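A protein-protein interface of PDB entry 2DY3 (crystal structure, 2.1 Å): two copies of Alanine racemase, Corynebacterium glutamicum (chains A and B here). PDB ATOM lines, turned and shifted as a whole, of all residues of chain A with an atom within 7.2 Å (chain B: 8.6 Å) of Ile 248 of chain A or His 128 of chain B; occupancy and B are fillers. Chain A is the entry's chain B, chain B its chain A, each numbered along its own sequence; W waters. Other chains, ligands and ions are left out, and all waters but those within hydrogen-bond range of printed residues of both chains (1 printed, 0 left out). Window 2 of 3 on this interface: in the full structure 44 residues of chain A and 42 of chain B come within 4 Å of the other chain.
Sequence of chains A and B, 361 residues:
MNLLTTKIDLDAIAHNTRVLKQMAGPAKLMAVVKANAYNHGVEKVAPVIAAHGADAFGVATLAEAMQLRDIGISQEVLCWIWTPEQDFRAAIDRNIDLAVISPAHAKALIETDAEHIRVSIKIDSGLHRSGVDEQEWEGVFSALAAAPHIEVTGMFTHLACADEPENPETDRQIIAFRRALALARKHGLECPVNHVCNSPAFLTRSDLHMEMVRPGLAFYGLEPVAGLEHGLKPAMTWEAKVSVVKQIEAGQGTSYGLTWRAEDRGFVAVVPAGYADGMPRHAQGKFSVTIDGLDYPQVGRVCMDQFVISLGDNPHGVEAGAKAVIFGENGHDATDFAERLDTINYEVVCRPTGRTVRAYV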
ATOM      1  N   LYS A 246     -11.636 -10.852  -9.414  1.00  0.00           N
ATOM      2  CA  LYS A 246     -11.906 -11.033  -7.994  1.00  0.00           C
ATOM      3  C   LYS A 246     -11.169 -10.036  -7.115  1.00  0.00           C
ATOM      4  O   LYS A 246     -10.004  -9.729  -7.351  1.00  0.00           O
ATOM      5  CB  LYS A 246     -11.503 -12.450  -7.580  1.00  0.00           C
ATOM      6  CG  LYS A 246     -12.280 -13.022  -6.409  1.00  0.00           C
ATOM      7  CD  LYS A 246     -13.741 -13.205  -6.785  1.00  0.00           C
ATOM      8  CE  LYS A 246     -14.370 -14.330  -6.000  1.00  0.00           C
ATOM      9  NZ  LYS A 246     -13.821 -15.640  -6.423  1.00  0.00           N
ATOM     10  N   GLN A 247     -11.855  -9.533  -6.099  1.00  0.00           N
ATOM     11  CA  GLN A 247     -11.234  -8.603  -5.175  1.00  0.00           C
ATOM     12  C   GLN A 247     -10.858  -9.361  -3.916  1.00  0.00           C
ATOM     13  O   GLN A 247     -11.660 -10.122  -3.377  1.00  0.00           O
ATOM     14  CB  GLN A 247     -12.183  -7.463  -4.809  1.00  0.00           C
ATOM     15  CG  GLN A 247     -11.567  -6.495  -3.803  1.00  0.00           C
ATOM     16  CD  GLN A 247     -12.431  -5.281  -3.525  1.00  0.00           C
ATOM     17  OE1 GLN A 247     -12.044  -4.398  -2.759  1.00  0.00           O
ATOM     18  NE2 GLN A 247     -13.606  -5.228  -4.148  1.00  0.00           N
ATOM     19  N   ILE A 248      -9.628  -9.165  -3.464  1.00  0.00           N
ATOM     20  CA  ILE A 248      -9.155  -9.811  -2.252  1.00  0.00           C
ATOM     21  C   ILE A 248      -9.176  -8.745  -1.169  1.00  0.00           C
ATOM     22  O   ILE A 248      -8.187  -8.048  -0.951  1.00  0.00           O
ATOM     23  CB  ILE A 248      -7.721 -10.337  -2.419  1.00  0.00           C
ATOM     24  CG1 ILE A 248      -7.663 -11.305  -3.603  1.00  0.00           C
ATOM     25  CG2 ILE A 248      -7.265 -11.027  -1.139  1.00  0.00           C
ATOM     26  CD1 ILE A 248      -6.273 -11.804  -3.917  1.00  0.00           C
ATOM     27  N   ARG A 265      -6.482  -3.353  -0.772  1.00  0.00           N
ATOM     28  CA  ARG A 265      -7.635  -3.490  -1.653  1.00  0.00           C
ATOM     29  C   ARG A 265      -7.096  -4.019  -2.975  1.00  0.00           C
ATOM     30  O   ARG A 265      -6.966  -3.276  -3.949  1.00  0.00           O
ATOM     31  CB  ARG A 265      -8.328  -2.146  -1.882  1.00  0.00           C
ATOM     32  CG  ARG A 265      -9.712  -2.298  -2.495  1.00  0.00           C
ATOM     33  CD  ARG A 265     -10.194  -1.032  -3.177  1.00  0.00           C
ATOM     34  NE  ARG A 265     -11.498  -1.238  -3.803  1.00  0.00           N
ATOM     35  CZ  ARG A 265     -12.000  -0.466  -4.760  1.00  0.00           C
ATOM     36  NH1 ARG A 265     -11.304   0.569  -5.212  1.00  0.00           N
ATOM     37  NH2 ARG A 265     -13.195  -0.733  -5.270  1.00  0.00           N
ATOM     38  N   GLY A 266      -6.766  -5.306  -2.992  1.00  0.00           N
ATOM     39  CA  GLY A 266      -6.226  -5.915  -4.189  1.00  0.00           C
ATOM     40  C   GLY A 266      -7.250  -6.675  -5.004  1.00  0.00           C
ATOM     41  O   GLY A 266      -8.344  -6.983  -4.535  1.00  0.00           O
ATOM     42  N   PHE A 267      -6.881  -6.975  -6.239  1.00  0.00           N
ATOM     43  CA  PHE A 267      -7.747  -7.697  -7.148  1.00  0.00           C
ATOM     44  C   PHE A 267      -6.900  -8.660  -7.970  1.00  0.00           C
ATOM     45  O   PHE A 267      -5.708  -8.431  -8.182  1.00  0.00           O
ATOM     46  CB  PHE A 267      -8.435  -6.726  -8.113  1.00  0.00           C
ATOM     47  CG  PHE A 267      -9.275  -5.683  -7.441  1.00  0.00           C
ATOM     48  CD1 PHE A 267     -10.650  -5.836  -7.345  1.00  0.00           C
ATOM     49  CD2 PHE A 267      -8.694  -4.535  -6.926  1.00  0.00           C
ATOM     50  CE1 PHE A 267     -11.432  -4.860  -6.749  1.00  0.00           C
ATOM     51  CE2 PHE A 267      -9.465  -3.557  -6.328  1.00  0.00           C
ATOM     52  CZ  PHE A 267     -10.840  -3.720  -6.240  1.00  0.00           C
ATOM     53  N   VAL A 268      -7.529  -9.738  -8.422  1.00  0.00           N
ATOM     54  CA  VAL A 268      -6.883 -10.721  -9.276  1.00  0.00           C
ATOM     55  C   VAL A 268      -7.893 -10.982 -10.377  1.00  0.00           C
ATOM     56  O   VAL A 268      -9.079 -10.689 -10.220  1.00  0.00           O
ATOM     57  CB  VAL A 268      -6.585 -12.068  -8.549  1.00  0.00           C
ATOM     58  CG1 VAL A 268      -5.621 -11.841  -7.407  1.00  0.00           C
ATOM     59  CG2 VAL A 268      -7.874 -12.712  -8.065  1.00  0.00           C
ATOM     60  N   ALA A 269      -7.418 -11.513 -11.496  1.00  0.00           N
ATOM     61  CA  ALA A 269      -8.286 -11.833 -12.617  1.00  0.00           C
ATOM     62  C   ALA A 269      -7.994 -13.267 -13.041  1.00  0.00           C
ATOM     63  O   ALA A 269      -6.852 -13.725 -12.985  1.00  0.00           O
ATOM     64  CB  ALA A 269      -8.035 -10.867 -13.785  1.00  0.00           C
ATOM     65  N   VAL A 270      -9.037 -13.980 -13.441  1.00  0.00           N
ATOM     66  CA  VAL A 270      -8.879 -15.355 -13.878  1.00  0.00           C
ATOM     67  C   VAL A 270      -8.921 -15.399 -15.399  1.00  0.00           C
ATOM     68  O   VAL A 270      -9.820 -14.835 -16.012  1.00  0.00           O
ATOM     69  CB  VAL A 270     -10.008 -16.245 -13.318  1.00  0.00           C
ATOM     70  CG1 VAL A 270      -9.797 -17.691 -13.747  1.00  0.00           C
ATOM     71  CG2 VAL A 270     -10.033 -16.148 -11.794  1.00  0.00           C
ATOM     72  N   VAL A 308      -4.052 -17.377 -12.805  1.00  0.00           N
ATOM     73  CA  VAL A 308      -4.449 -16.080 -12.274  1.00  0.00           C
ATOM     74  C   VAL A 308      -3.384 -15.008 -12.446  1.00  0.00           C
ATOM     75  O   VAL A 308      -2.184 -15.298 -12.470  1.00  0.00           O
ATOM     76  CB  VAL A 308      -4.776 -16.206 -10.760  1.00  0.00           C
ATOM     77  CG1 VAL A 308      -5.442 -14.942 -10.250  1.00  0.00           C
ATOM     78  CG2 VAL A 308      -5.653 -17.427 -10.526  1.00  0.00           C
ATOM     79  N   GLY A 312      -3.353  -5.814  -8.893  1.00  0.00           N
ATOM     80  CA  GLY A 312      -2.967  -4.837  -7.891  1.00  0.00           C
ATOM     81  C   GLY A 312      -4.258  -4.195  -7.421  1.00  0.00           C
ATOM     82  O   GLY A 312      -5.216  -4.901  -7.102  1.00  0.00           O
ATOM     83  N   ILE B 123     -18.891 -21.699  -5.230  1.00  0.00           N
ATOM     84  CA  ILE B 123     -18.504 -20.940  -4.054  1.00  0.00           C
ATOM     85  C   ILE B 123     -17.006 -20.716  -3.913  1.00  0.00           C
ATOM     86  O   ILE B 123     -16.215 -21.650  -4.017  1.00  0.00           O
ATOM     87  CB  ILE B 123     -19.006 -21.639  -2.762  1.00  0.00           C
ATOM     88  CG1 ILE B 123     -20.537 -21.693  -2.742  1.00  0.00           C
ATOM     89  CG2 ILE B 123     -18.474 -20.923  -1.547  1.00  0.00           C
ATOM     90  CD1 ILE B 123     -21.225 -20.339  -2.787  1.00  0.00           C
ATOM     91  N   ASP B 124     -16.620 -19.465  -3.704  1.00  0.00           N
ATOM     92  CA  ASP B 124     -15.215 -19.154  -3.480  1.00  0.00           C
ATOM     93  C   ASP B 124     -15.060 -19.445  -1.991  1.00  0.00           C
ATOM     94  O   ASP B 124     -15.522 -18.670  -1.162  1.00  0.00           O
ATOM     95  CB  ASP B 124     -14.924 -17.675  -3.752  1.00  0.00           C
ATOM     96  CG  ASP B 124     -13.476 -17.299  -3.456  1.00  0.00           C
ATOM     97  OD1 ASP B 124     -12.812 -18.032  -2.688  1.00  0.00           O
ATOM     98  OD2 ASP B 124     -13.004 -16.262  -3.981  1.00  0.00           O
ATOM     99  N   SER B 125     -14.439 -20.569  -1.659  1.00  0.00           N
ATOM    100  CA  SER B 125     -14.257 -20.952  -0.264  1.00  0.00           C
ATOM    101  C   SER B 125     -12.899 -20.560   0.318  1.00  0.00           C
ATOM    102  O   SER B 125     -12.460 -21.136   1.309  1.00  0.00           O
ATOM    103  CB  SER B 125     -14.468 -22.463  -0.100  1.00  0.00           C
ATOM    104  OG  SER B 125     -13.641 -23.207  -0.979  1.00  0.00           O
ATOM    105  N   GLY B 126     -12.237 -19.581  -0.290  1.00  0.00           N
ATOM    106  CA  GLY B 126     -10.949 -19.159   0.231  1.00  0.00           C
ATOM    107  C   GLY B 126      -9.828 -19.074  -0.782  1.00  0.00           C
ATOM    108  O   GLY B 126      -8.855 -18.362  -0.563  1.00  0.00           O
ATOM    109  N   LEU B 127      -9.951 -19.796  -1.892  1.00  0.00           N
ATOM    110  CA  LEU B 127      -8.919 -19.779  -2.920  1.00  0.00           C
ATOM    111  C   LEU B 127      -8.845 -18.443  -3.647  1.00  0.00           C
ATOM    112  O   LEU B 127      -7.794 -18.072  -4.175  1.00  0.00           O
ATOM    113  CB  LEU B 127      -9.158 -20.904  -3.930  1.00  0.00           C
ATOM    114  CG  LEU B 127      -8.581 -22.265  -3.540  1.00  0.00           C
ATOM    115  CD1 LEU B 127      -8.821 -22.515  -2.071  1.00  0.00           C
ATOM    116  CD2 LEU B 127      -9.196 -23.354  -4.387  1.00  0.00           C
ATOM    117  N   HIS B 128      -9.961 -17.727  -3.691  1.00  0.00           N
ATOM    118  CA  HIS B 128      -9.993 -16.429  -4.353  1.00  0.00           C
ATOM    119  C   HIS B 128      -9.731 -16.469  -5.856  1.00  0.00           C
ATOM    120  O   HIS B 128      -9.063 -15.585  -6.389  1.00  0.00           O
ATOM    121  CB  HIS B 128      -8.985 -15.484  -3.695  1.00  0.00           C
ATOM    122  CG  HIS B 128      -9.325 -15.134  -2.280  1.00  0.00           C
ATOM    123  ND1 HIS B 128      -8.397 -14.635  -1.393  1.00  0.00           N
ATOM    124  CD2 HIS B 128     -10.496 -15.198  -1.602  1.00  0.00           C
ATOM    125  CE1 HIS B 128      -8.980 -14.407  -0.230  1.00  0.00           C
ATOM    126  NE2 HIS B 128     -10.254 -14.740  -0.330  1.00  0.00           N
ATOM    127  N   ARG B 129     -10.172 -17.512  -6.498  1.00  0.00           N
ATOM    128  CA  ARG B 129     -10.135 -17.587  -7.951  1.00  0.00           C
ATOM    129  C   ARG B 129     -11.491 -17.261  -8.562  1.00  0.00           C
ATOM    130  O   ARG B 129     -11.971 -16.162  -8.232  1.00  0.00           O
ATOM    131  CB  ARG B 129      -9.693 -18.975  -8.410  1.00  0.00           C
ATOM    132  CG  ARG B 129      -8.479 -19.520  -7.680  1.00  0.00           C
ATOM    133  CD  ARG B 129      -7.563 -20.262  -8.636  1.00  0.00           C
ATOM    134  NE  ARG B 129      -6.216 -19.707  -8.651  1.00  0.00           N
ATOM    135  CZ  ARG B 129      -5.185 -20.272  -9.269  1.00  0.00           C
ATOM    136  NH1 ARG B 129      -5.352 -21.413  -9.926  1.00  0.00           N
ATOM    137  NH2 ARG B 129      -3.992 -19.696  -9.234  1.00  0.00           N
ATOM    138  N   SER B 130     -12.137 -18.182  -9.197  1.00  0.00           N
ATOM    139  CA  SER B 130     -13.487 -17.893  -9.671  1.00  0.00           C
ATOM    140  C   SER B 130     -14.471 -18.304  -8.574  1.00  0.00           C
ATOM    141  O   SER B 130     -14.062 -18.806  -7.525  1.00  0.00           O
ATOM    142  CB  SER B 130     -13.801 -18.631 -10.984  1.00  0.00           C
ATOM    143  OG  SER B 130     -14.089 -20.001 -10.776  1.00  0.00           O
ATOM    144  N   GLY B 131     -15.758 -18.082  -8.809  1.00  0.00           N
ATOM    145  CA  GLY B 131     -16.752 -18.417  -7.805  1.00  0.00           C
ATOM    146  C   GLY B 131     -17.146 -17.180  -7.013  1.00  0.00           C
ATOM    147  O   GLY B 131     -16.405 -16.194  -6.980  1.00  0.00           O
ATOM    148  N   VAL B 132     -18.309 -17.230  -6.372  1.00  0.00           N
ATOM    149  CA  VAL B 132     -18.819 -16.110  -5.585  1.00  0.00           C
ATOM    150  C   VAL B 132     -18.197 -16.124  -4.188  1.00  0.00           C
ATOM    151  O   VAL B 132     -18.165 -17.167  -3.540  1.00  0.00           O
ATOM    152  CB  VAL B 132     -20.354 -16.205  -5.459  1.00  0.00           C
ATOM    153  CG1 VAL B 132     -20.923 -14.902  -4.951  1.00  0.00           C
ATOM    154  CG2 VAL B 132     -20.960 -16.560  -6.803  1.00  0.00           C
ATOM    155  N   ASP B 133     -17.684 -14.983  -3.730  1.00  0.00           N
ATOM    156  CA  ASP B 133     -17.078 -14.935  -2.406  1.00  0.00           C
ATOM    157  C   ASP B 133     -18.073 -14.565  -1.312  1.00  0.00           C
ATOM    158  O   ASP B 133     -19.201 -14.162  -1.591  1.00  0.00           O
ATOM    159  CB  ASP B 133     -15.871 -13.986  -2.370  1.00  0.00           C
ATOM    160  CG  ASP B 133     -16.210 -12.569  -2.788  1.00  0.00           C
ATOM    161  OD1 ASP B 133     -17.215 -12.004  -2.305  1.00  0.00           O
ATOM    162  OD2 ASP B 133     -15.449 -12.010  -3.598  1.00  0.00           O
ATOM    163  N   GLU B 134     -17.642 -14.726  -0.065  1.00  0.00           N
ATOM    164  CA  GLU B 134     -18.485 -14.451   1.088  1.00  0.00           C
ATOM    165  C   GLU B 134     -19.172 -13.094   1.053  1.00  0.00           C
ATOM    166  O   GLU B 134     -20.358 -12.990   1.369  1.00  0.00           O
ATOM    167  CB  GLU B 134     -17.682 -14.600   2.386  1.00  0.00           C
ATOM    168  CG  GLU B 134     -18.556 -14.580   3.638  1.00  0.00           C
ATOM    169  CD  GLU B 134     -17.918 -15.273   4.827  1.00  0.00           C
ATOM    170  OE1 GLU B 134     -18.599 -15.409   5.862  1.00  0.00           O
ATOM    171  OE2 GLU B 134     -16.741 -15.684   4.734  1.00  0.00           O
ATOM    172  N   GLN B 135     -18.446 -12.054   0.660  1.00  0.00           N
ATOM    173  CA  GLN B 135     -19.037 -10.723   0.597  1.00  0.00           C
ATOM    174  C   GLN B 135     -20.194 -10.683  -0.398  1.00  0.00           C
ATOM    175  O   GLN B 135     -21.063  -9.811  -0.320  1.00  0.00           O
ATOM    176  CB  GLN B 135     -17.985  -9.686   0.197  1.00  0.00           C
ATOM    177  CG  GLN B 135     -16.830  -9.551   1.179  1.00  0.00           C
ATOM    178  CD  GLN B 135     -16.035 -10.835   1.326  1.00  0.00           C
ATOM    179  OE1 GLN B 135     -15.510 -11.368   0.345  1.00  0.00           O
ATOM    180  NE2 GLN B 135     -15.941 -11.340   2.555  1.00  0.00           N
ATOM    181  N   THR B 157     -17.628 -26.210  -4.469  1.00  0.00           N
ATOM    182  CA  THR B 157     -16.397 -25.445  -4.354  1.00  0.00           C
ATOM    183  C   THR B 157     -15.263 -26.410  -4.705  1.00  0.00           C
ATOM    184  O   THR B 157     -15.477 -27.619  -4.769  1.00  0.00           O
ATOM    185  CB  THR B 157     -16.203 -24.906  -2.927  1.00  0.00           C
ATOM    186  OG1 THR B 157     -15.222 -23.858  -2.935  1.00  0.00           O
ATOM    187  CG2 THR B 157     -15.748 -26.022  -2.003  1.00  0.00           C
ATOM    188  N   HIS B 158     -14.067 -25.884  -4.934  1.00  0.00           N
ATOM    189  CA  HIS B 158     -12.940 -26.730  -5.302  1.00  0.00           C
ATOM    190  C   HIS B 158     -11.813 -26.641  -4.269  1.00  0.00           C
ATOM    191  O   HIS B 158     -11.386 -25.550  -3.900  1.00  0.00           O
ATOM    192  CB  HIS B 158     -12.443 -26.321  -6.691  1.00  0.00           C
ATOM    193  CG  HIS B 158     -11.590 -27.353  -7.358  1.00  0.00           C
ATOM    194  ND1 HIS B 158     -11.916 -28.693  -7.370  1.00  0.00           N
ATOM    195  CD2 HIS B 158     -10.441 -27.239  -8.063  1.00  0.00           C
ATOM    196  CE1 HIS B 158     -11.003 -29.359  -8.054  1.00  0.00           C
ATOM    197  NE2 HIS B 158     -10.097 -28.500  -8.485  1.00  0.00           N
ATOM    198  N   GLU B 169      -6.687 -25.696   5.544  1.00  0.00           N
ATOM    199  CA  GLU B 169      -6.985 -25.384   4.152  1.00  0.00           C
ATOM    200  C   GLU B 169      -8.199 -26.158   3.660  1.00  0.00           C
ATOM    201  O   GLU B 169      -9.252 -25.571   3.427  1.00  0.00           O
ATOM    202  CB  GLU B 169      -5.792 -25.664   3.244  1.00  0.00           C
ATOM    203  CG  GLU B 169      -5.867 -24.833   1.982  1.00  0.00           C
ATOM    204  CD  GLU B 169      -6.337 -23.421   2.283  1.00  0.00           C
ATOM    205  OE1 GLU B 169      -5.730 -22.765   3.156  1.00  0.00           O
ATOM    206  OE2 GLU B 169      -7.312 -22.965   1.651  1.00  0.00           O
ATOM    207  N   GLN B 173     -11.527 -24.611   3.967  1.00  0.00           N
ATOM    208  CA  GLN B 173     -12.425 -24.323   2.856  1.00  0.00           C
ATOM    209  C   GLN B 173     -13.796 -24.915   3.155  1.00  0.00           C
ATOM    210  O   GLN B 173     -14.820 -24.341   2.801  1.00  0.00           O
ATOM    211  CB  GLN B 173     -11.896 -24.931   1.556  1.00  0.00           C
ATOM    212  CG  GLN B 173     -10.615 -24.318   1.033  1.00  0.00           C
ATOM    213  CD  GLN B 173     -10.264 -24.839  -0.346  1.00  0.00           C
ATOM    214  OE1 GLN B 173     -10.984 -24.591  -1.317  1.00  0.00           O
ATOM    215  NE2 GLN B 173      -9.164 -25.575  -0.440  1.00  0.00           N
HETATM  216  O   HOH W   1      -2.179 -18.814 -11.613  1.00  0.00           O
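OD2 of Asp 124 of chain B lies within salt-bridge range of NZ of Lys 246 of chain A, 2.6 Å away.
The backbone carbonyl oxygen of Arg 129 of chain B is in hydrogen-bond range of the side-chain amino group of Lys 246 of chain A (2.6 Å).
The backbone carbonyl oxygen (O) of Ser 130 of chain B lies within hydrogen-bond range of the side-chain amino group (NZ) of Lys 246 of chain A (3.4 Å).
The backbone carbonyl oxygen of Gly 131 of chain B sits at hydrogen-bond distance from the side-chain amino group of Lys 246 of chain A.
OD1 of Asp 124 of chain B sits at hydrogen-bond distance from N of Gly 126 of chain B, at 2.9 Å.
The backbone NH (N) of His 128 of chain B is in hydrogen-bond range of the side-chain carboxylate (OD1) of Asp 124 of chain B (3.0 Å).
The backbone NH (N) of Asp 124 of chain B lies within hydrogen-bond range of the backbone carbonyl oxygen (O) of Val 132 of chain B, at 2.8 Å.
OD1 of Asp 133 of chain B sits at hydrogen-bond distance from N of Gln 135 of chain B (3.2 Å).
N of Lys 246 of chain A lies within hydrogen-bond range of O of Val 268 of chain A, 2.7 Å away.
O of Gly 266 of chain A is in hydrogen-bond range of N of Ile 248 of chain A (2.7 Å).
CE of Lys 246 of chain A touches OD2 of Asp 133 of chain B (3.5 Å).
ND1 of His 128 of chain B touches CG2 of Ile 248 of chain A (3.8 Å).
Val 268 of chain A touches His 128 of chain B.
Arg 129 of chain B touches Val 270 of chain A.
Val 270 of chain A touches Ser 130 of chain B (CG2 to N, 3.9 Å).
Val 308 of chain A touches Arg 129 of chain B (CG2 to NE, 3.0 Å).
Ile 248 of chain A touches just one residue of chain B: His 128.
No residue of chain B comes within 4 Å of Gly 266 of chain A.
Of the printed residues of chain B, Val 308 of chain A touches Arg 129 (3.0 Å).
Of the printed residues of chain A, Asp 124 of chain B touches Lys 246.
Of chain A, only Ile 248 (3.8 Å) and Val 268 (3.5 Å) come within 4 Å of His 128 of chain B.
Of the printed residues of chain A, Ser 130 of chain B touches Lys 246 and Val 270.
Val 132 of chain B touches none of the printed residues of chain A.
The nearest printed residue of chain B that does not touch Ile 248 of chain A is Leu 127 of chain B (6.5 Å).
Of the 11 printed residues of chain A, 5 touch a printed residue of chain B.
Printed residues of chain A that touch a printed residue of chain B: Lys 246, Ile 248, Val 268, Val 270 and Val 308.
Of the 17 printed residues of chain B, 6 touch a printed residue of chain A.
No position is printed for both chains.
Water W1 lies within hydrogen-bond range of the backbone NH (N) of Val 308 of chain A (2.6 Å) and the guanidinium group (NH2) of Arg 129 of chain B (3.1 Å).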
